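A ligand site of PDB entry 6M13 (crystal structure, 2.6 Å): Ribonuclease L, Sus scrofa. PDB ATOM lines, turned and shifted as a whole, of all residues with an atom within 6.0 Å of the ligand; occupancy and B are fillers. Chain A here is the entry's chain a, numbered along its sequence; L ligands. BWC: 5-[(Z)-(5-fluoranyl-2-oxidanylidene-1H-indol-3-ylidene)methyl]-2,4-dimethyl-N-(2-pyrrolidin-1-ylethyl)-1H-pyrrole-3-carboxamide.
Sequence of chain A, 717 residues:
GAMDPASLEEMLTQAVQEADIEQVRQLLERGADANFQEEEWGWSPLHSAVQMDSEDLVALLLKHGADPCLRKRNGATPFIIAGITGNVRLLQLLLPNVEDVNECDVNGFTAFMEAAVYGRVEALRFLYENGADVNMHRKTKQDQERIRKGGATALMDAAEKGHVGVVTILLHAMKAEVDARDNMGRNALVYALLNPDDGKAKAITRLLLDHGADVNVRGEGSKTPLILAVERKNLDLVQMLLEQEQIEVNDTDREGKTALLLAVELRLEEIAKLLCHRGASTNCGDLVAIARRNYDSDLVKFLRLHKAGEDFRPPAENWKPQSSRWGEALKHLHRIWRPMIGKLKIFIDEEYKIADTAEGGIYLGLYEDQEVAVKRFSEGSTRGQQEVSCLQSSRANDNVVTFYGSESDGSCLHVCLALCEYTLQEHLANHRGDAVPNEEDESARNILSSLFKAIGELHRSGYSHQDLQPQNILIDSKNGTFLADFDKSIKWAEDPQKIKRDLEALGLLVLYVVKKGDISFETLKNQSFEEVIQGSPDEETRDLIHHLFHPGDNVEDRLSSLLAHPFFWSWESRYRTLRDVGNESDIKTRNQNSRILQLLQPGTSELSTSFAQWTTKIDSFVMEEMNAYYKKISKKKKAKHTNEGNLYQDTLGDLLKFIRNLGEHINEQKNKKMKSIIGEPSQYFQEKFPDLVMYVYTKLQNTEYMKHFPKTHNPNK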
ATOM      1  N   ARG A 325       4.616   7.883  29.857  1.00  0.00           N
ATOM      2  CA  ARG A 325       5.753   8.453  29.124  1.00  0.00           C
ATOM      3  C   ARG A 325       5.609   9.969  28.925  1.00  0.00           C
ATOM      4  O   ARG A 325       6.556  10.707  29.144  1.00  0.00           O
ATOM      5  CB  ARG A 325       5.907   7.776  27.765  1.00  0.00           C
ATOM      6  CG  ARG A 325       7.007   8.386  26.918  1.00  0.00           C
ATOM      7  CD  ARG A 325       7.334   7.518  25.754  1.00  0.00           C
ATOM      8  NE  ARG A 325       8.456   8.017  24.983  1.00  0.00           N
ATOM      9  CZ  ARG A 325       8.784   7.617  23.760  1.00  0.00           C
ATOM     10  NH1 ARG A 325       8.050   6.721  23.118  1.00  0.00           N
ATOM     11  NH2 ARG A 325       9.845   8.139  23.165  1.00  0.00           N
ATOM     12  N   TRP A 326       4.419  10.401  28.520  1.00  0.00           N
ATOM     13  CA  TRP A 326       4.156  11.805  28.200  1.00  0.00           C
ATOM     14  C   TRP A 326       3.450  12.559  29.320  1.00  0.00           C
ATOM     15  O   TRP A 326       3.127  13.733  29.147  1.00  0.00           O
ATOM     16  CB  TRP A 326       3.291  11.872  26.929  1.00  0.00           C
ATOM     17  CG  TRP A 326       3.826  11.093  25.792  1.00  0.00           C
ATOM     18  CD1 TRP A 326       3.267   9.996  25.212  1.00  0.00           C
ATOM     19  CD2 TRP A 326       5.045  11.345  25.091  1.00  0.00           C
ATOM     20  NE1 TRP A 326       4.062   9.550  24.174  1.00  0.00           N
ATOM     21  CE2 TRP A 326       5.155  10.359  24.084  1.00  0.00           C
ATOM     22  CE3 TRP A 326       6.040  12.309  25.203  1.00  0.00           C
ATOM     23  CZ2 TRP A 326       6.240  10.317  23.199  1.00  0.00           C
ATOM     24  CZ3 TRP A 326       7.111  12.259  24.333  1.00  0.00           C
ATOM     25  CH2 TRP A 326       7.207  11.277  23.334  1.00  0.00           C
ATOM     26  N   ILE A 354       6.981  15.131  19.980  1.00  0.00           N
ATOM     27  CA  ILE A 354       7.010  13.673  20.029  1.00  0.00           C
ATOM     28  C   ILE A 354       8.036  13.151  19.055  1.00  0.00           C
ATOM     29  O   ILE A 354       8.807  12.272  19.403  1.00  0.00           O
ATOM     30  CB  ILE A 354       5.603  13.093  19.697  1.00  0.00           C
ATOM     31  CG1 ILE A 354       4.617  13.484  20.767  1.00  0.00           C
ATOM     32  CG2 ILE A 354       5.643  11.562  19.627  1.00  0.00           C
ATOM     33  CD1 ILE A 354       3.198  13.055  20.504  1.00  0.00           C
ATOM     34  N   ALA A 355       8.022  13.671  17.829  1.00  0.00           N
ATOM     35  CA  ALA A 355       8.849  13.180  16.752  1.00  0.00           C
ATOM     36  C   ALA A 355       8.964  14.186  15.590  1.00  0.00           C
ATOM     37  O   ALA A 355       8.256  15.195  15.561  1.00  0.00           O
ATOM     38  CB  ALA A 355       8.214  11.904  16.234  1.00  0.00           C
ATOM     39  N   ASP A 356       9.854  13.894  14.649  1.00  0.00           N
ATOM     40  CA  ASP A 356      10.104  14.752  13.471  1.00  0.00           C
ATOM     41  C   ASP A 356       9.455  14.149  12.256  1.00  0.00           C
ATOM     42  O   ASP A 356       9.372  12.920  12.159  1.00  0.00           O
ATOM     43  CB  ASP A 356      11.612  14.863  13.238  1.00  0.00           C
ATOM     44  CG  ASP A 356      12.315  15.671  14.308  1.00  0.00           C
ATOM     45  OD1 ASP A 356      12.369  16.898  14.126  1.00  0.00           O
ATOM     46  OD2 ASP A 356      12.796  15.089  15.324  1.00  0.00           O
ATOM     47  N   ILE A 362       5.511  15.978  15.012  1.00  0.00           N
ATOM     48  CA  ILE A 362       4.439  15.427  15.832  1.00  0.00           C
ATOM     49  C   ILE A 362       4.556  16.032  17.200  1.00  0.00           C
ATOM     50  O   ILE A 362       5.608  15.924  17.811  1.00  0.00           O
ATOM     51  CB  ILE A 362       4.533  13.890  15.968  1.00  0.00           C
ATOM     52  CG1 ILE A 362       4.694  13.210  14.589  1.00  0.00           C
ATOM     53  CG2 ILE A 362       3.317  13.340  16.699  1.00  0.00           C
ATOM     54  CD1 ILE A 362       3.450  13.061  13.748  1.00  0.00           C
ATOM     55  N   ALA A 373      -1.854  13.164  19.924  1.00  0.00           N
ATOM     56  CA  ALA A 373      -0.675  13.453  19.118  1.00  0.00           C
ATOM     57  C   ALA A 373      -1.132  14.229  17.924  1.00  0.00           C
ATOM     58  O   ALA A 373      -2.128  13.876  17.324  1.00  0.00           O
ATOM     59  CB  ALA A 373      -0.003  12.167  18.678  1.00  0.00           C
ATOM     60  N   LYS A 375      -0.276  15.771  14.330  1.00  0.00           N
ATOM     61  CA  LYS A 375       0.551  15.783  13.140  1.00  0.00           C
ATOM     62  C   LYS A 375       0.154  16.991  12.300  1.00  0.00           C
ATOM     63  O   LYS A 375      -1.014  17.174  11.968  1.00  0.00           O
ATOM     64  CB  LYS A 375       0.340  14.506  12.336  1.00  0.00           C
ATOM     65  CG  LYS A 375       1.283  14.356  11.163  1.00  0.00           C
ATOM     66  CD  LYS A 375       1.189  12.923  10.638  1.00  0.00           C
ATOM     67  CE  LYS A 375       2.276  12.625   9.623  1.00  0.00           C
ATOM     68  NZ  LYS A 375       1.886  11.424   8.855  1.00  0.00           N
ATOM     69  N   VAL A 401      -4.766   3.855  14.329  1.00  0.00           N
ATOM     70  CA  VAL A 401      -4.722   4.775  15.439  1.00  0.00           C
ATOM     71  C   VAL A 401      -5.981   5.618  15.403  1.00  0.00           C
ATOM     72  O   VAL A 401      -6.421   6.042  14.333  1.00  0.00           O
ATOM     73  CB  VAL A 401      -3.447   5.640  15.347  1.00  0.00           C
ATOM     74  CG1 VAL A 401      -3.511   6.576  14.119  1.00  0.00           C
ATOM     75  CG2 VAL A 401      -3.223   6.407  16.633  1.00  0.00           C
ATOM     76  N   LEU A 417      -4.525  12.709  16.770  1.00  0.00           N
ATOM     77  CA  LEU A 417      -4.621  11.261  16.835  1.00  0.00           C
ATOM     78  C   LEU A 417      -4.454  10.779  18.263  1.00  0.00           C
ATOM     79  O   LEU A 417      -3.898  11.474  19.097  1.00  0.00           O
ATOM     80  CB  LEU A 417      -3.542  10.616  15.984  1.00  0.00           C
ATOM     81  CG  LEU A 417      -3.405  11.184  14.584  1.00  0.00           C
ATOM     82  CD1 LEU A 417      -2.003  10.952  14.015  1.00  0.00           C
ATOM     83  CD2 LEU A 417      -4.485  10.598  13.669  1.00  0.00           C
ATOM     84  N   ALA A 418      -4.904   9.571  18.527  1.00  0.00           N
ATOM     85  CA  ALA A 418      -4.672   8.950  19.816  1.00  0.00           C
ATOM     86  C   ALA A 418      -3.180   8.908  20.112  1.00  0.00           C
ATOM     87  O   ALA A 418      -2.358   8.550  19.262  1.00  0.00           O
ATOM     88  CB  ALA A 418      -5.261   7.532  19.857  1.00  0.00           C
ATOM     89  N   LEU A 419      -2.847   9.257  21.350  1.00  0.00           N
ATOM     90  CA  LEU A 419      -1.464   9.239  21.800  1.00  0.00           C
ATOM     91  C   LEU A 419      -1.111   7.827  22.215  1.00  0.00           C
ATOM     92  O   LEU A 419      -1.821   7.218  23.017  1.00  0.00           O
ATOM     93  CB  LEU A 419      -1.322  10.165  23.000  1.00  0.00           C
ATOM     94  CG  LEU A 419       0.059  10.438  23.527  1.00  0.00           C
ATOM     95  CD1 LEU A 419       0.912  11.057  22.438  1.00  0.00           C
ATOM     96  CD2 LEU A 419      -0.041  11.334  24.766  1.00  0.00           C
ATOM     97  N   CYS A 420      -0.030   7.305  21.676  1.00  0.00           N
ATOM     98  CA  CYS A 420       0.444   5.983  22.052  1.00  0.00           C
ATOM     99  C   CYS A 420       1.750   6.120  22.807  1.00  0.00           C
ATOM    100  O   CYS A 420       2.426   7.168  22.717  1.00  0.00           O
ATOM    101  CB  CYS A 420       0.643   5.142  20.801  1.00  0.00           C
ATOM    102  SG  CYS A 420      -0.906   4.877  19.923  1.00  0.00           S
ATOM    103  N   GLU A 421       2.115   5.058  23.547  1.00  0.00           N
ATOM    104  CA  GLU A 421       3.307   5.106  24.385  1.00  0.00           C
ATOM    105  C   GLU A 421       4.568   5.072  23.512  1.00  0.00           C
ATOM    106  O   GLU A 421       5.329   6.019  23.496  1.00  0.00           O
ATOM    107  CB  GLU A 421       3.343   3.982  25.392  1.00  0.00           C
ATOM    108  CG  GLU A 421       2.328   4.147  26.509  1.00  0.00           C
ATOM    109  CD  GLU A 421       2.729   5.256  27.476  1.00  0.00           C
ATOM    110  OE1 GLU A 421       3.521   4.984  28.412  1.00  0.00           O
ATOM    111  OE2 GLU A 421       2.240   6.386  27.281  1.00  0.00           O
ATOM    112  N   TYR A 422       4.746   3.984  22.769  1.00  0.00           N
ATOM    113  CA  TYR A 422       5.984   3.688  22.085  1.00  0.00           C
ATOM    114  C   TYR A 422       5.760   3.310  20.626  1.00  0.00           C
ATOM    115  O   TYR A 422       4.731   2.782  20.252  1.00  0.00           O
ATOM    116  CB  TYR A 422       6.710   2.539  22.797  1.00  0.00           C
ATOM    117  CG  TYR A 422       7.097   2.869  24.214  1.00  0.00           C
ATOM    118  CD1 TYR A 422       8.199   3.694  24.489  1.00  0.00           C
ATOM    119  CD2 TYR A 422       6.358   2.372  25.296  1.00  0.00           C
ATOM    120  CE1 TYR A 422       8.576   3.998  25.788  1.00  0.00           C
ATOM    121  CE2 TYR A 422       6.696   2.696  26.602  1.00  0.00           C
ATOM    122  CZ  TYR A 422       7.824   3.491  26.852  1.00  0.00           C
ATOM    123  OH  TYR A 422       8.188   3.828  28.136  1.00  0.00           O
ATOM    124  N   THR A 423       6.781   3.569  19.836  1.00  0.00           N
ATOM    125  CA  THR A 423       6.924   3.001  18.501  1.00  0.00           C
ATOM    126  C   THR A 423       7.185   1.512  18.650  1.00  0.00           C
ATOM    127  O   THR A 423       7.633   1.042  19.695  1.00  0.00           O
ATOM    128  CB  THR A 423       8.091   3.734  17.797  1.00  0.00           C
ATOM    129  OG1 THR A 423       7.586   4.935  17.232  1.00  0.00           O
ATOM    130  CG2 THR A 423       8.785   2.967  16.757  1.00  0.00           C
ATOM    131  N   GLN A 425       9.642  -0.114  17.222  1.00  0.00           N
ATOM    132  CA  GLN A 425      11.100  -0.120  17.501  1.00  0.00           C
ATOM    133  C   GLN A 425      11.438   0.080  18.992  1.00  0.00           C
ATOM    134  O   GLN A 425      12.173  -0.664  19.561  1.00  0.00           O
ATOM    135  CB  GLN A 425      11.777   0.972  16.668  1.00  0.00           C
ATOM    136  CG  GLN A 425      13.259   0.947  16.512  1.00  0.00           C
ATOM    137  CD  GLN A 425      13.685   2.031  15.497  1.00  0.00           C
ATOM    138  OE1 GLN A 425      14.330   2.980  15.875  1.00  0.00           O
ATOM    139  NE2 GLN A 425      13.274   1.892  14.224  1.00  0.00           N
ATOM    140  N   GLU A 426      10.869   1.081  19.611  1.00  0.00           N
ATOM    141  CA  GLU A 426      11.158   1.342  21.014  1.00  0.00           C
ATOM    142  C   GLU A 426      10.600   0.175  21.862  1.00  0.00           C
ATOM    143  O   GLU A 426      11.210  -0.292  22.796  1.00  0.00           O
ATOM    144  CB  GLU A 426      10.519   2.670  21.455  1.00  0.00           C
ATOM    145  CG  GLU A 426      11.026   3.911  20.717  1.00  0.00           C
ATOM    146  CD  GLU A 426      10.139   5.134  20.899  1.00  0.00           C
ATOM    147  OE1 GLU A 426       8.903   4.980  20.913  1.00  0.00           O
ATOM    148  OE2 GLU A 426      10.656   6.276  21.007  1.00  0.00           O
ATOM    149  N   GLN A 471       8.542   2.665  12.342  1.00  0.00           N
ATOM    150  CA  GLN A 471       8.204   3.959  12.974  1.00  0.00           C
ATOM    151  C   GLN A 471       6.745   4.379  12.716  1.00  0.00           C
ATOM    152  O   GLN A 471       6.241   5.195  13.461  1.00  0.00           O
ATOM    153  CB  GLN A 471       9.201   5.062  12.678  1.00  0.00           C
ATOM    154  CG  GLN A 471       9.694   5.131  11.252  1.00  0.00           C
ATOM    155  CD  GLN A 471      10.881   4.158  10.999  1.00  0.00           C
ATOM    156  OE1 GLN A 471      10.686   2.982  10.612  1.00  0.00           O
ATOM    157  NE2 GLN A 471      12.102   4.637  11.209  1.00  0.00           N
ATOM    158  N   ASN A 472       6.063   3.766  11.748  1.00  0.00           N
ATOM    159  CA  ASN A 472       4.637   3.952  11.516  1.00  0.00           C
ATOM    160  C   ASN A 472       3.749   3.015  12.295  1.00  0.00           C
ATOM    161  O   ASN A 472       2.551   2.942  12.000  1.00  0.00           O
ATOM    162  CB  ASN A 472       4.334   3.743  10.019  1.00  0.00           C
ATOM    163  CG  ASN A 472       5.082   4.744   9.162  1.00  0.00           C
ATOM    164  OD1 ASN A 472       5.447   5.823   9.624  1.00  0.00           O
ATOM    165  ND2 ASN A 472       5.340   4.378   7.934  1.00  0.00           N
ATOM    166  N   LEU A 474       2.595   1.870  16.209  1.00  0.00           N
ATOM    167  CA  LEU A 474       2.639   2.367  17.577  1.00  0.00           C
ATOM    168  C   LEU A 474       2.019   1.384  18.558  1.00  0.00           C
ATOM    169  O   LEU A 474       1.090   0.651  18.215  1.00  0.00           O
ATOM    170  CB  LEU A 474       1.902   3.680  17.631  1.00  0.00           C
ATOM    171  CG  LEU A 474       2.193   4.652  16.513  1.00  0.00           C
ATOM    172  CD1 LEU A 474       1.243   5.807  16.635  1.00  0.00           C
ATOM    173  CD2 LEU A 474       3.626   5.146  16.584  1.00  0.00           C
ATOM    174  N   ALA A 484      -0.207   3.731  11.991  1.00  0.00           N
ATOM    175  CA  ALA A 484      -0.399   5.169  11.831  1.00  0.00           C
ATOM    176  C   ALA A 484       0.297   5.690  10.562  1.00  0.00           C
ATOM    177  O   ALA A 484       0.882   4.912   9.806  1.00  0.00           O
ATOM    178  CB  ALA A 484       0.082   5.905  13.039  1.00  0.00           C
ATOM    179  N   ASP A 485       0.203   6.986  10.357  1.00  0.00           N
ATOM    180  CA  ASP A 485       0.904   7.737   9.285  1.00  0.00           C
ATOM    181  C   ASP A 485       0.480   7.481   7.830  1.00  0.00           C
ATOM    182  O   ASP A 485       1.218   6.960   7.056  1.00  0.00           O
ATOM    183  CB  ASP A 485       2.425   7.636   9.428  1.00  0.00           C
ATOM    184  CG  ASP A 485       2.949   8.267  10.677  1.00  0.00           C
ATOM    185  OD1 ASP A 485       2.395   9.271  11.181  1.00  0.00           O
ATOM    186  OD2 ASP A 485       3.984   7.762  11.183  1.00  0.00           O
HETATM  187  OAK BWC L   1       5.432   8.692  13.937  1.00  0.00           O
HETATM  188  CAI BWC L   1       4.504   8.759  14.783  1.00  0.00           C
HETATM  189  NAH BWC L   1       3.217   8.961  14.406  1.00  0.00           N
HETATM  190  CAD BWC L   1       2.447   8.984  15.526  1.00  0.00           C
HETATM  191  CAC BWC L   1       1.120   9.173  15.687  1.00  0.00           C
HETATM  192  CAB BWC L   1       0.552   9.119  16.970  1.00  0.00           C
HETATM  193  CAA BWC L   1       1.362   8.904  18.080  1.00  0.00           C
HETATM  194  FAG BWC L   1       0.815   8.856  19.360  1.00  0.00           F
HETATM  195  CAF BWC L   1       2.740   8.729  17.882  1.00  0.00           C
HETATM  196  CAE BWC L   1       3.268   8.774  16.630  1.00  0.00           C
HETATM  197  CAJ BWC L   1       4.561   8.643  16.166  1.00  0.00           C
HETATM  198  CAL BWC L   1       5.607   8.394  17.063  1.00  0.00           C
HETATM  199  CAM BWC L   1       6.975   8.379  16.818  1.00  0.00           C
HETATM  200  CAQ BWC L   1       7.968   8.349  17.765  1.00  0.00           C
HETATM  201  CAR BWC L   1       7.660   8.350  19.303  1.00  0.00           C
HETATM  202  NAN BWC L   1       7.589   8.364  15.610  1.00  0.00           N
HETATM  203  CAO BWC L   1       8.925   8.330  15.817  1.00  0.00           C
HETATM  204  CAS BWC L   1       9.920   8.333  14.610  1.00  0.00           C
HETATM  205  CAP BWC L   1       9.210   8.344  17.168  1.00  0.00           C
HETATM  206  CAT BWC L   1      10.475   8.287  17.750  1.00  0.00           C
HETATM  207  OAU BWC L   1      10.970   7.166  17.918  1.00  0.00           O
HETATM  208  NAV BWC L   1      11.118   9.470  18.141  1.00  0.00           N
HETATM  209  CAW BWC L   1      12.498   9.616  18.657  1.00  0.00           C
HETATM  210  CAX BWC L   1      12.807   8.762  19.897  1.00  0.00           C
HETATM  211  NAY BWC L   1      13.581   7.539  19.666  1.00  0.00           N
HETATM  212  CAZ BWC L   1      13.489   6.721  18.438  1.00  0.00           C
HETATM  213  CBA BWC L   1      14.924   6.620  17.943  1.00  0.00           C
HETATM  214  CBB BWC L   1      15.772   6.959  19.119  1.00  0.00           C
HETATM  215  CBC BWC L   1      14.968   8.085  19.646  1.00  0.00           C
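A fluorine (FAG) of the ligand sits close to the backbone carbonyl oxygen (O) of Ala 418, 3.2 Å away.
N of Cys 420 sits close to FAG of the ligand, at 2.9 Å.
Residues that only touch the ligand: Leu 419 (3.4 Å), Leu 474 (3.4 Å), Thr 423 (3.5 Å), Ala 373 (3.5 Å), Gln 471 (3.6 Å), Ala 355 (3.6 Å), Ile 354 (3.8 Å) and Leu 417 (3.96 Å).
Hydrophobic or aromatic side chains within 4 Å of the ligand: Ile 354, Ala 355, Ala 373, Leu 417, Leu 419 and Leu 474.
The nearest printed residue that does not touch the ligand is Ile 362 (4.2 Å).
The side-chain carboxylate of Asp 485 sits close to the side-chain amide oxygen of Asn 472 (2.9 Å).
O of Ala 373 sits at hydrogen-bond distance from N of Leu 417.
The side-chain carboxylate (OD1) of Asp 485 is in salt-bridge range of the side-chain amino group (NZ) of Lys 375 (3.2 Å).
The guanidinium group (NH1) of Arg 325 lies within salt-bridge range of the side-chain carboxylate (OE1) of Glu 426, at 2.9 Å.
The backbone carbonyl oxygen (O) of Cys 420 sits at hydrogen-bond distance from the indole nitrogen (NE1) of Trp 326 (3.2 Å).
The backbone NH (N) of Ile 354 sits at hydrogen-bond distance from the backbone carbonyl oxygen (O) of Ile 362 (2.7 Å).
N of Ile 362 is in hydrogen-bond range of O of Ala 355 (2.9 Å).
OE1 of Glu 426 lies within hydrogen-bond range of N of Thr 423.
The side-chain carboxylate (OD1) of Asp 485 sits at hydrogen-bond distance from a nitrogen (NAH) of the ligand.
A nitrogen (NAY) of the ligand lies within salt-bridge range of the side-chain carboxylate of Glu 426 (3.5 Å).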
